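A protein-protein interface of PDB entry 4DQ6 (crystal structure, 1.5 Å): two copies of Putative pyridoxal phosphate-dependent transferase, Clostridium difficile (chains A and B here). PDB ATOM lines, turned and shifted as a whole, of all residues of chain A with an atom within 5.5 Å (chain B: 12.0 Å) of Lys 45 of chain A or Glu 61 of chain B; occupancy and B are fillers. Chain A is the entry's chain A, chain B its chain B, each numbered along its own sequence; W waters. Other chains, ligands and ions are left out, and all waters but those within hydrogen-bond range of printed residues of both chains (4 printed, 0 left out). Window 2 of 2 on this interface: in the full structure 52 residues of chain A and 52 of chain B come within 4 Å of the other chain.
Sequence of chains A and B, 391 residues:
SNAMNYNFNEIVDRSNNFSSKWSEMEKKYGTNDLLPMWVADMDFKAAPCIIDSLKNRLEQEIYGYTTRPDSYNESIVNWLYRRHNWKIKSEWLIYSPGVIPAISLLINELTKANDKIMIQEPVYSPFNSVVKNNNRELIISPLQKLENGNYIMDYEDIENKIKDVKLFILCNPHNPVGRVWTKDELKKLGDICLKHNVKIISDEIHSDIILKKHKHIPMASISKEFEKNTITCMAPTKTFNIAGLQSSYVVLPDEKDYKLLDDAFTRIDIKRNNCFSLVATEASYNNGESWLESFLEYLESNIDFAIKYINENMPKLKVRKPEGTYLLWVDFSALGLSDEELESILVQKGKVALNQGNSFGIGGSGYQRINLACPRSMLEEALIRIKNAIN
NH1 of Arg 57 of chain B lies close to ND2 of Asn 17 of chain A (3.3 Å). The side-chain amide oxygen (OE1) of Gln 60 of chain B sits at hydrogen-bond distance from the side-chain amide nitrogen (ND2) of Asn 17 of chain A (2.9 Å). O of Ile 62 of chain B sits at hydrogen-bond distance from ND2 of Asn 17 of chain A (3.0 Å). OE1 of Glu 61 of chain B lies within salt-bridge range of NZ of Lys 45 of chain A (3.0 Å). The backbone NH (N) of Ala 46 of chain A sits at hydrogen-bond distance from the backbone carbonyl oxygen (O) of Glu 61 of chain B (2.9 Å). O of Asn 241 of chain A sits close to O of Tyr 63 of chain B (3.4 Å).
The side-chain amino group of Lys 45 of chain A lies within salt-bridge range of the side-chain carboxylate of Glu 10 of chain A (3.4 Å). The side-chain amide nitrogen (ND2) of Asn 241 of chain A is in hydrogen-bond range of the backbone carbonyl oxygen (O) of Phe 44 of chain A, at 3.1 Å. The guanidinium group of Arg 57 of chain B sits close to the side-chain amide oxygen of Gln 60 of chain B, 3.4 Å away. The guanidinium group (NH2) of Arg 57 of chain B lies within hydrogen-bond range of the backbone carbonyl oxygen (O) of Ile 62 of chain B (2.9 Å). OH of Tyr 63 of chain B lies within hydrogen-bond range of O of Leu 58 of chain B (2.6 Å).
Ile 62 of chain B touches Val 12 of chain A (CD1 to CG1, 3.8 Å). O of Phe 44 of chain A touches CG1 of Ile 62 of chain B (3.6 Å). CA of Lys 45 of chain A touches CG1 of Ile 62 of chain B (3.9 Å). Tyr 63 of chain B touches Ala 46 of chain A. Ile 51 of chain A touches Leu 58 of chain B (CG2 to CD2, 3.97 Å). CD1 of Ile 51 of chain A touches CG of Glu 61 of chain B, 3.6 Å away. Tyr 63 of chain B touches Ile 51 of chain A (OH to CG1, 3.9 Å). Lys 55 of chain A touches Leu 58 of chain B. Ile 62 of chain B touches Asn 241 of chain A.
Lys 45 of chain A touches two residues of chain B. Of the printed residues of chain A, Glu 61 of chain B touches Lys 45, Ala 46 and Ile 51. Phe 44 of chain A touches just one residue of chain B: Ile 62 (3.6 Å). No residue of chain B comes within 4 Å of Ala 47 of chain A. Of chain B, only Leu 58, Glu 61 and Tyr 63 come within 4 Å of Ile 51 of chain A. Of the printed residues of chain B, Asn 241 of chain A touches Ile 62 and Tyr 63. Of the printed residues of chain B, Lys 55 of chain A touches Leu 58 (3.4 Å). Of the printed residues of chain A, Ile 62 of chain B touches Val 12 (3.8 Å), Asn 17 (3.0 Å), Phe 44 (3.6 Å), Lys 45 (3.9 Å) and Asn 241 (3.97 Å). Of the printed residues of chain B, Asn 17 of chain A touches Arg 57, Gln 60 and Ile 62. Of the printed residues of chain A, Tyr 63 of chain B touches Ala 46, Ile 51 and Asn 241. Of the printed residues of chain A, Arg 57 of chain B touches Asn 17. Asp 43 of chain A touches none of the printed residues of chain B. Thr 66 of chain B touches none of the printed residues of chain A. The nearest residue of chain A that does not touch Glu 61 of chain B is Phe 44 of chain A (4.6 Å).
Printed residues of chain A that touch a printed residue of chain B: Val 12, Asn 17, Phe 44, Lys 45, Ala 46, Ile 51, Lys 55 and Asn 241. Hydrophobic or aromatic side chains of chain A that line the printed part of chain B: Val 12, Ala 46 and Ile 51. Of the 18 printed residues of chain B, 6 touch a printed residue of chain A. Hydrophobic or aromatic side chains of chain B that line the printed part of chain A: Leu 58, Ile 62 and Tyr 63. Among the printed residues, 15 pairs touch across the chains. Among the printed residues, Asp or Glu carboxylates within 4 Å of a Lys or Arg side-chain nitrogen of the other chain: Lys 45 of chain A with Glu 61 of chain B (3.0 Å).
Position printed for both chains: 55. Of the 15 pairs that touch across the chains among the printed residues, none has its exchanged pair printed and touching as well.
Water W4 bridges the backbone carbonyl oxygen (O) of Asn 241 of chain A and the backbone NH (N) of Tyr 63 of chain B. Water W2 lies within hydrogen-bond range of OD1 of Asn 17 of chain A, N of Gly 64 of chain B, NH2 of Arg 57 of chain B and O of Ile 62 of chain B. Water W1 lies within hydrogen-bond range of OE2 of Glu 61 of chain B (2.8 Å) and NZ of Lys 55 of chain A (3.1 Å). Water W3 lies within hydrogen-bond range of the side-chain hydroxyl (OG1) of Thr 66 of chain B, the guanidinium group (NH2) of Arg 57 of chain B, the backbone carbonyl oxygen (O) of Asn 17 of chain A and the backbone carbonyl oxygen (O) of Gly 64 of chain B.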
ATOM      1  N   GLU A  10      21.599   0.995  12.002  1.00  0.00           N
ATOM      2  CA  GLU A  10      20.710   2.141  11.890  1.00  0.00           C
ATOM      3  C   GLU A  10      21.432   3.457  12.180  1.00  0.00           C
ATOM      4  O   GLU A  10      22.046   3.577  13.188  1.00  0.00           O
ATOM      5  CB  GLU A  10      19.520   1.984  12.881  1.00  0.00           C
ATOM      6  CG  GLU A  10      18.535   3.165  12.859  1.00  0.00           C
ATOM      7  CD  GLU A  10      17.283   2.974  13.731  1.00  0.00           C
ATOM      8  OE1 GLU A  10      17.286   2.173  14.688  1.00  0.00           O
ATOM      9  OE2 GLU A  10      16.274   3.659  13.448  1.00  0.00           O
ATOM     10  N   VAL A  12      21.396   6.928  14.036  1.00  0.00           N
ATOM     11  CA  VAL A  12      20.533   7.606  15.033  1.00  0.00           C
ATOM     12  C   VAL A  12      21.166   8.979  15.307  1.00  0.00           C
ATOM     13  O   VAL A  12      22.137   9.111  16.053  1.00  0.00           O
ATOM     14  CB  VAL A  12      20.285   6.787  16.349  1.00  0.00           C
ATOM     15  CG1 VAL A  12      19.007   7.250  17.034  1.00  0.00           C
ATOM     16  CG2 VAL A  12      20.159   5.287  16.084  1.00  0.00           C
ATOM     17  N   ASN A  17      19.638  15.253  20.983  1.00  0.00           N
ATOM     18  CA  ASN A  17      19.740  14.300  22.117  1.00  0.00           C
ATOM     19  C   ASN A  17      20.579  14.878  23.290  1.00  0.00           C
ATOM     20  O   ASN A  17      20.934  14.094  24.166  1.00  0.00           O
ATOM     21  CB  ASN A  17      20.339  13.000  21.502  1.00  0.00           C
ATOM     22  CG  ASN A  17      20.506  11.820  22.439  1.00  0.00           C
ATOM     23  OD1 ASN A  17      21.614  11.245  22.514  1.00  0.00           O
ATOM     24  ND2 ASN A  17      19.441  11.371  23.092  1.00  0.00           N
ATOM     25  N   ASP A  43      27.012   5.522  19.826  1.00  0.00           N
ATOM     26  CA  ASP A  43      25.932   6.012  18.942  1.00  0.00           C
ATOM     27  C   ASP A  43      24.999   4.874  18.560  1.00  0.00           C
ATOM     28  O   ASP A  43      24.624   4.650  17.358  1.00  0.00           O
ATOM     29  CB  ASP A  43      26.499   6.659  17.705  1.00  0.00           C
ATOM     30  CG  ASP A  43      27.161   7.990  18.006  1.00  0.00           C
ATOM     31  OD1 ASP A  43      26.441   8.968  18.305  1.00  0.00           O
ATOM     32  OD2 ASP A  43      28.400   8.074  17.933  1.00  0.00           O
ATOM     33  N   PHE A  44      24.598   4.179  19.599  1.00  0.00           N
ATOM     34  CA  PHE A  44      23.623   3.127  19.511  1.00  0.00           C
ATOM     35  C   PHE A  44      22.484   3.345  20.505  1.00  0.00           C
ATOM     36  O   PHE A  44      22.658   3.861  21.541  1.00  0.00           O
ATOM     37  CB  PHE A  44      24.213   1.782  19.829  1.00  0.00           C
ATOM     38  CG  PHE A  44      25.253   1.317  18.882  1.00  0.00           C
ATOM     39  CD1 PHE A  44      25.106   1.375  17.504  1.00  0.00           C
ATOM     40  CD2 PHE A  44      26.377   0.748  19.396  1.00  0.00           C
ATOM     41  CE1 PHE A  44      26.141   0.938  16.675  1.00  0.00           C
ATOM     42  CE2 PHE A  44      27.393   0.260  18.600  1.00  0.00           C
ATOM     43  CZ  PHE A  44      27.276   0.390  17.213  1.00  0.00           C
ATOM     44  N   LYS A  45      21.280   2.930  20.161  1.00  0.00           N
ATOM     45  CA  LYS A  45      20.171   2.898  21.104  1.00  0.00           C
ATOM     46  C   LYS A  45      20.439   1.975  22.256  1.00  0.00           C
ATOM     47  O   LYS A  45      21.151   0.980  22.107  1.00  0.00           O
ATOM     48  CB  LYS A  45      18.901   2.438  20.403  1.00  0.00           C
ATOM     49  CG  LYS A  45      18.375   3.477  19.442  1.00  0.00           C
ATOM     50  CD  LYS A  45      17.088   3.016  18.841  1.00  0.00           C
ATOM     51  CE  LYS A  45      16.581   4.095  17.922  1.00  0.00           C
ATOM     52  NZ  LYS A  45      15.424   3.499  17.224  1.00  0.00           N
ATOM     53  N   ALA A  46      19.897   2.269  23.418  1.00  0.00           N
ATOM     54  CA  ALA A  46      20.023   1.364  24.550  1.00  0.00           C
ATOM     55  C   ALA A  46      19.286   0.098  24.251  1.00  0.00           C
ATOM     56  O   ALA A  46      18.379   0.109  23.408  1.00  0.00           O
ATOM     57  CB  ALA A  46      19.418   1.998  25.832  1.00  0.00           C
ATOM     58  N   ALA A  47      19.581  -0.970  24.933  1.00  0.00           N
ATOM     59  CA  ALA A  47      18.887  -2.217  24.788  1.00  0.00           C
ATOM     60  C   ALA A  47      17.383  -2.077  24.981  1.00  0.00           C
ATOM     61  O   ALA A  47      16.919  -1.289  25.794  1.00  0.00           O
ATOM     62  CB  ALA A  47      19.406  -3.241  25.765  1.00  0.00           C
ATOM     63  N   ILE A  51      15.014   0.433  27.620  1.00  0.00           N
ATOM     64  CA  ILE A  51      14.012   1.419  27.209  1.00  0.00           C
ATOM     65  C   ILE A  51      12.661   1.047  27.848  1.00  0.00           C
ATOM     66  O   ILE A  51      11.971   1.919  28.386  1.00  0.00           O
ATOM     67  CB  ILE A  51      13.926   1.516  25.686  1.00  0.00           C
ATOM     68  CG1 ILE A  51      15.264   1.946  25.077  1.00  0.00           C
ATOM     69  CG2 ILE A  51      12.822   2.488  25.264  1.00  0.00           C
ATOM     70  CD1 ILE A  51      15.324   1.675  23.577  1.00  0.00           C
ATOM     71  N   LYS A  55      10.275   3.165  30.356  1.00  0.00           N
ATOM     72  CA  LYS A  55       8.913   3.524  30.039  1.00  0.00           C
ATOM     73  C   LYS A  55       7.976   3.155  31.146  1.00  0.00           C
ATOM     74  O   LYS A  55       7.165   3.973  31.532  1.00  0.00           O
ATOM     75  CB  LYS A  55       8.448   2.857  28.737  1.00  0.00           C
ATOM     76  CG  LYS A  55       9.157   3.382  27.522  1.00  0.00           C
ATOM     77  CD  LYS A  55       8.580   2.631  26.321  1.00  0.00           C
ATOM     78  CE  LYS A  55       9.182   3.042  24.996  1.00  0.00           C
ATOM     79  NZ  LYS A  55       8.614   2.208  23.889  1.00  0.00           N
ATOM     80  N   ASN A 241      25.642   1.752  27.550  1.00  0.00           N
ATOM     81  CA  ASN A 241      25.430   3.107  27.038  1.00  0.00           C
ATOM     82  C   ASN A 241      24.412   3.911  27.801  1.00  0.00           C
ATOM     83  O   ASN A 241      23.483   4.520  27.168  1.00  0.00           O
ATOM     84  CB  ASN A 241      25.025   3.078  25.576  1.00  0.00           C
ATOM     85  CG  ASN A 241      25.277   4.388  24.883  1.00  0.00           C
ATOM     86  OD1 ASN A 241      26.126   5.184  25.268  1.00  0.00           O
ATOM     87  ND2 ASN A 241      24.602   4.579  23.810  1.00  0.00           N
ATOM     88  N   TRP A 291      21.456  -8.588  24.251  1.00  0.00           N
ATOM     89  CA  TRP A 291      21.928  -7.343  23.625  1.00  0.00           C
ATOM     90  C   TRP A 291      23.418  -7.167  23.743  1.00  0.00           C
ATOM     91  O   TRP A 291      24.081  -6.864  22.728  1.00  0.00           O
ATOM     92  CB  TRP A 291      21.152  -6.138  24.171  1.00  0.00           C
ATOM     93  CG  TRP A 291      21.540  -4.875  23.499  1.00  0.00           C
ATOM     94  CD1 TRP A 291      20.939  -4.252  22.380  1.00  0.00           C
ATOM     95  CD2 TRP A 291      22.676  -4.014  23.866  1.00  0.00           C
ATOM     96  NE1 TRP A 291      21.605  -3.102  22.082  1.00  0.00           N
ATOM     97  CE2 TRP A 291      22.659  -2.905  22.918  1.00  0.00           C
ATOM     98  CE3 TRP A 291      23.666  -4.053  24.839  1.00  0.00           C
ATOM     99  CZ2 TRP A 291      23.562  -1.886  22.959  1.00  0.00           C
ATOM    100  CZ3 TRP A 291      24.569  -3.011  24.877  1.00  0.00           C
ATOM    101  CH2 TRP A 291      24.541  -1.959  23.943  1.00  0.00           C
ATOM    102  N   ASP B  52       5.523  14.934  29.938  1.00  0.00           N
ATOM    103  CA  ASP B  52       5.717  14.861  28.521  1.00  0.00           C
ATOM    104  C   ASP B  52       7.168  15.144  28.118  1.00  0.00           C
ATOM    105  O   ASP B  52       7.646  14.538  27.155  1.00  0.00           O
ATOM    106  CB  ASP B  52       4.823  15.850  27.829  1.00  0.00           C
ATOM    107  CG  ASP B  52       4.453  15.380  26.423  1.00  0.00           C
ATOM    108  OD1 ASP B  52       3.865  14.259  26.237  1.00  0.00           O
ATOM    109  OD2 ASP B  52       4.934  16.055  25.517  1.00  0.00           O
ATOM    110  N   SER B  53       7.886  16.029  28.863  1.00  0.00           N
ATOM    111  CA  SER B  53       9.312  16.294  28.578  1.00  0.00           C
ATOM    112  C   SER B  53      10.186  14.998  28.776  1.00  0.00           C
ATOM    113  O   SER B  53      11.010  14.654  27.934  1.00  0.00           O
ATOM    114  CB  SER B  53       9.922  17.449  29.426  1.00  0.00           C
ATOM    115  OG  SER B  53      10.321  17.096  30.804  1.00  0.00           O
ATOM    116  N   LEU B  54       9.851  14.244  29.825  1.00  0.00           N
ATOM    117  CA  LEU B  54      10.459  12.949  30.041  1.00  0.00           C
ATOM    118  C   LEU B  54      10.206  11.966  28.946  1.00  0.00           C
ATOM    119  O   LEU B  54      11.129  11.287  28.513  1.00  0.00           O
ATOM    120  CB  LEU B  54       9.987  12.394  31.388  1.00  0.00           C
ATOM    121  CG  LEU B  54      10.384  13.178  32.642  1.00  0.00           C
ATOM    122  CD1 LEU B  54       9.656  12.555  33.844  1.00  0.00           C
ATOM    123  CD2 LEU B  54      11.890  13.236  32.791  1.00  0.00           C
ATOM    124  N   LYS B  55       8.948  11.906  28.503  1.00  0.00           N
ATOM    125  CA  LYS B  55       8.497  11.042  27.328  1.00  0.00           C
ATOM    126  C   LYS B  55       9.247  11.350  26.070  1.00  0.00           C
ATOM    127  O   LYS B  55       9.797  10.458  25.421  1.00  0.00           O
ATOM    128  CB  LYS B  55       7.010  11.119  27.072  1.00  0.00           C
ATOM    129  CG  LYS B  55       6.251  10.344  28.120  1.00  0.00           C
ATOM    130  CD  LYS B  55       4.817  10.203  27.696  1.00  0.00           C
ATOM    131  CE  LYS B  55       3.894  10.010  28.877  1.00  0.00           C
ATOM    132  NZ  LYS B  55       2.495  10.246  28.436  1.00  0.00           N
ATOM    133  N   ASN B  56       9.343  12.623  25.741  1.00  0.00           N
ATOM    134  CA  ASN B  56      10.067  13.016  24.558  1.00  0.00           C
ATOM    135  C   ASN B  56      11.533  12.621  24.680  1.00  0.00           C
ATOM    136  O   ASN B  56      12.109  12.067  23.750  1.00  0.00           O
ATOM    137  CB  ASN B  56       9.927  14.522  24.328  1.00  0.00           C
ATOM    138  CG  ASN B  56      10.761  15.004  23.163  1.00  0.00           C
ATOM    139  OD1 ASN B  56      10.326  14.905  22.011  1.00  0.00           O
ATOM    140  ND2 ASN B  56      11.931  15.575  23.460  1.00  0.00           N
ATOM    141  N   ARG B  57      12.111  12.818  25.859  1.00  0.00           N
ATOM    142  CA  ARG B  57      13.489  12.449  25.981  1.00  0.00           C
ATOM    143  C   ARG B  57      13.689  10.935  25.942  1.00  0.00           C
ATOM    144  O   ARG B  57      14.696  10.432  25.381  1.00  0.00           O
ATOM    145  CB  ARG B  57      14.127  13.027  27.277  1.00  0.00           C
ATOM    146  CG  ARG B  57      15.620  12.775  27.498  1.00  0.00           C
ATOM    147  CD  ARG B  57      16.519  13.341  26.404  1.00  0.00           C
ATOM    148  NE  ARG B  57      17.928  12.974  26.593  1.00  0.00           N
ATOM    149  CZ  ARG B  57      18.390  11.787  26.214  1.00  0.00           C
ATOM    150  NH1 ARG B  57      17.579  10.850  25.714  1.00  0.00           N
ATOM    151  NH2 ARG B  57      19.662  11.509  26.361  1.00  0.00           N
ATOM    152  N   LEU B  58      12.835  10.204  26.648  1.00  0.00           N
ATOM    153  CA  LEU B  58      12.912   8.764  26.633  1.00  0.00           C
ATOM    154  C   LEU B  58      12.913   8.200  25.217  1.00  0.00           C
ATOM    155  O   LEU B  58      13.725   7.330  24.854  1.00  0.00           O
ATOM    156  CB  LEU B  58      11.739   8.193  27.436  1.00  0.00           C
ATOM    157  CG  LEU B  58      11.831   6.684  27.712  1.00  0.00           C
ATOM    158  CD1 LEU B  58      11.180   6.442  29.079  1.00  0.00           C
ATOM    159  CD2 LEU B  58      11.280   5.913  26.553  1.00  0.00           C
ATOM    160  N   GLU B  59      11.963   8.717  24.409  1.00  0.00           N
ATOM    161  CA  GLU B  59      11.711   8.205  23.039  1.00  0.00           C
ATOM    162  C   GLU B  59      12.865   8.465  22.045  1.00  0.00           C
ATOM    163  O   GLU B  59      12.901   7.910  20.969  1.00  0.00           O
ATOM    164  CB  GLU B  59      10.379   8.735  22.528  1.00  0.00           C
ATOM    165  CG  GLU B  59       9.224   8.175  23.340  1.00  0.00           C
ATOM    166  CD  GLU B  59       7.876   8.682  22.896  1.00  0.00           C
ATOM    167  OE1 GLU B  59       7.827   9.577  22.029  1.00  0.00           O
ATOM    168  OE2 GLU B  59       6.872   8.157  23.421  1.00  0.00           O
ATOM    169  N   GLN B  60      13.833   9.264  22.460  1.00  0.00           N
ATOM    170  CA  GLN B  60      15.143   9.386  21.722  1.00  0.00           C
ATOM    171  C   GLN B  60      16.007   8.121  21.803  1.00  0.00           C
ATOM    172  O   GLN B  60      16.806   7.863  20.898  1.00  0.00           O
ATOM    173  CB  GLN B  60      15.943  10.573  22.184  1.00  0.00           C
ATOM    174  CG  GLN B  60      15.219  11.894  21.914  1.00  0.00           C
ATOM    175  CD  GLN B  60      15.991  13.102  22.412  1.00  0.00           C
ATOM    176  OE1 GLN B  60      17.000  12.977  23.119  1.00  0.00           O
ATOM    177  NE2 GLN B  60      15.464  14.306  22.117  1.00  0.00           N
ATOM    178  N   GLU B  61      15.811   7.338  22.863  1.00  0.00           N
ATOM    179  CA  GLU B  61      16.384   6.015  23.055  1.00  0.00           C
ATOM    180  C   GLU B  61      17.911   5.909  23.184  1.00  0.00           C
ATOM    181  O   GLU B  61      18.441   4.775  23.140  1.00  0.00           O
ATOM    182  CB  GLU B  61      15.846   5.075  21.948  1.00  0.00           C
ATOM    183  CG  GLU B  61      14.350   4.837  22.077  1.00  0.00           C
ATOM    184  CD  GLU B  61      13.705   3.994  20.973  1.00  0.00           C
ATOM    185  OE1 GLU B  61      14.085   4.108  19.787  1.00  0.00           O
ATOM    186  OE2 GLU B  61      12.695   3.296  21.290  1.00  0.00           O
ATOM    187  N   ILE B  62      18.626   7.037  23.385  1.00  0.00           N
ATOM    188  CA  ILE B  62      20.074   7.005  23.674  1.00  0.00           C
ATOM    189  C   ILE B  62      20.256   7.853  24.908  1.00  0.00           C
ATOM    190  O   ILE B  62      19.755   9.006  24.972  1.00  0.00           O
ATOM    191  CB  ILE B  62      20.870   7.572  22.494  1.00  0.00           C
ATOM    192  CG1 ILE B  62      20.514   6.736  21.236  1.00  0.00           C
ATOM    193  CG2 ILE B  62      22.339   7.697  22.867  1.00  0.00           C
ATOM    194  CD1 ILE B  62      21.394   6.998  19.982  1.00  0.00           C
ATOM    195  N   TYR B  63      20.970   7.303  25.879  1.00  0.00           N
ATOM    196  CA  TYR B  63      21.065   7.918  27.182  1.00  0.00           C
ATOM    197  C   TYR B  63      22.534   8.084  27.584  1.00  0.00           C
ATOM    198  O   TYR B  63      22.973   7.589  28.630  1.00  0.00           O
ATOM    199  CB  TYR B  63      20.252   7.119  28.238  1.00  0.00           C
ATOM    200  CG  TYR B  63      18.886   6.749  27.737  1.00  0.00           C
ATOM    201  CD1 TYR B  63      17.844   7.696  27.591  1.00  0.00           C
ATOM    202  CD2 TYR B  63      18.619   5.436  27.458  1.00  0.00           C
ATOM    203  CE1 TYR B  63      16.644   7.327  27.013  1.00  0.00           C
ATOM    204  CE2 TYR B  63      17.402   5.038  26.944  1.00  0.00           C
ATOM    205  CZ  TYR B  63      16.416   6.010  26.772  1.00  0.00           C
ATOM    206  OH  TYR B  63      15.212   5.665  26.213  1.00  0.00           O
ATOM    207  N   GLY B  64      23.309   8.764  26.749  1.00  0.00           N
ATOM    208  CA  GLY B  64      24.739   8.989  27.004  1.00  0.00           C
ATOM    209  C   GLY B  64      25.005  10.267  27.732  1.00  0.00           C
ATOM    210  O   GLY B  64      24.156  10.868  28.372  1.00  0.00           O
ATOM    211  N   TYR B  65      26.285  10.679  27.736  1.00  0.00           N
ATOM    212  CA  TYR B  65      26.630  11.863  28.477  1.00  0.00           C
ATOM    213  C   TYR B  65      25.949  13.118  28.042  1.00  0.00           C
ATOM    214  O   TYR B  65      25.855  13.398  26.834  1.00  0.00           O
ATOM    215  CB  TYR B  65      28.161  12.088  28.359  1.00  0.00           C
ATOM    216  CG  TYR B  65      29.030  11.068  29.088  1.00  0.00           C
ATOM    217  CD1 TYR B  65      29.098  11.060  30.450  1.00  0.00           C
ATOM    218  CD2 TYR B  65      29.726  10.101  28.389  1.00  0.00           C
ATOM    219  CE1 TYR B  65      29.906  10.149  31.132  1.00  0.00           C
ATOM    220  CE2 TYR B  65      30.515   9.145  29.067  1.00  0.00           C
ATOM    221  CZ  TYR B  65      30.599   9.195  30.407  1.00  0.00           C
ATOM    222  OH  TYR B  65      31.338   8.253  31.106  1.00  0.00           O
ATOM    223  N   THR B  66      25.341  13.837  29.002  1.00  0.00           N
ATOM    224  CA  THR B  66      24.455  14.929  28.750  1.00  0.00           C
ATOM    225  C   THR B  66      25.080  16.300  28.869  1.00  0.00           C
ATOM    226  O   THR B  66      25.735  16.605  29.905  1.00  0.00           O
ATOM    227  CB  THR B  66      23.225  14.793  29.677  1.00  0.00           C
ATOM    228  OG1 THR B  66      22.670  13.472  29.488  1.00  0.00           O
ATOM    229  CG2 THR B  66      22.099  15.870  29.406  1.00  0.00           C
ATOM    230  N   CYS B 275      20.261  12.729  32.208  1.00  0.00           N
ATOM    231  CA  CYS B 275      19.540  13.175  30.990  1.00  0.00           C
ATOM    232  C   CYS B 275      18.072  13.583  31.235  1.00  0.00           C
ATOM    233  O   CYS B 275      17.470  14.387  30.487  1.00  0.00           O
ATOM    234  CB  CYS B 275      19.693  12.160  29.853  1.00  0.00           C
ATOM    235  SG  CYS B 275      18.987  10.575  30.213  1.00  0.00           S
ATOM    236  N   PHE B 276      17.446  12.987  32.244  1.00  0.00           N
ATOM    237  CA  PHE B 276      16.048  13.298  32.551  1.00  0.00           C
ATOM    238  C   PHE B 276      15.871  14.552  33.390  1.00  0.00           C
ATOM    239  O   PHE B 276      14.992  15.346  33.208  1.00  0.00           O
ATOM    240  CB  PHE B 276      15.364  12.062  33.137  1.00  0.00           C
ATOM    241  CG  PHE B 276      15.165  10.960  32.119  1.00  0.00           C
ATOM    242  CD1 PHE B 276      14.290  11.131  31.023  1.00  0.00           C
ATOM    243  CD2 PHE B 276      15.822   9.736  32.231  1.00  0.00           C
ATOM    244  CE1 PHE B 276      14.177  10.145  30.126  1.00  0.00           C
ATOM    245  CE2 PHE B 276      15.670   8.745  31.315  1.00  0.00           C
ATOM    246  CZ  PHE B 276      14.793   8.944  30.251  1.00  0.00           C
ATOM    247  N   VAL B 279      15.929  17.771  31.122  1.00  0.00           N
ATOM    248  CA  VAL B 279      14.753  18.200  30.417  1.00  0.00           C
ATOM    249  C   VAL B 279      13.623  18.540  31.349  1.00  0.00           C
ATOM    250  O   VAL B 279      12.867  19.478  31.077  1.00  0.00           O
ATOM    251  CB  VAL B 279      14.312  17.168  29.345  1.00  0.00           C
ATOM    252  CG1 VAL B 279      15.403  16.925  28.303  1.00  0.00           C
ATOM    253  CG2 VAL B 279      13.727  15.878  29.929  1.00  0.00           C
HETATM  254  O   HOH W   1      10.490   4.422  22.684  1.00  0.00           O
HETATM  255  O   HOH W   2      22.674  10.916  24.950  1.00  0.00           O
HETATM  256  O   HOH W   3      22.053  13.077  26.722  1.00  0.00           O
HETATM  257  O   HOH W   4      21.696   4.558  25.373  1.00  0.00           O
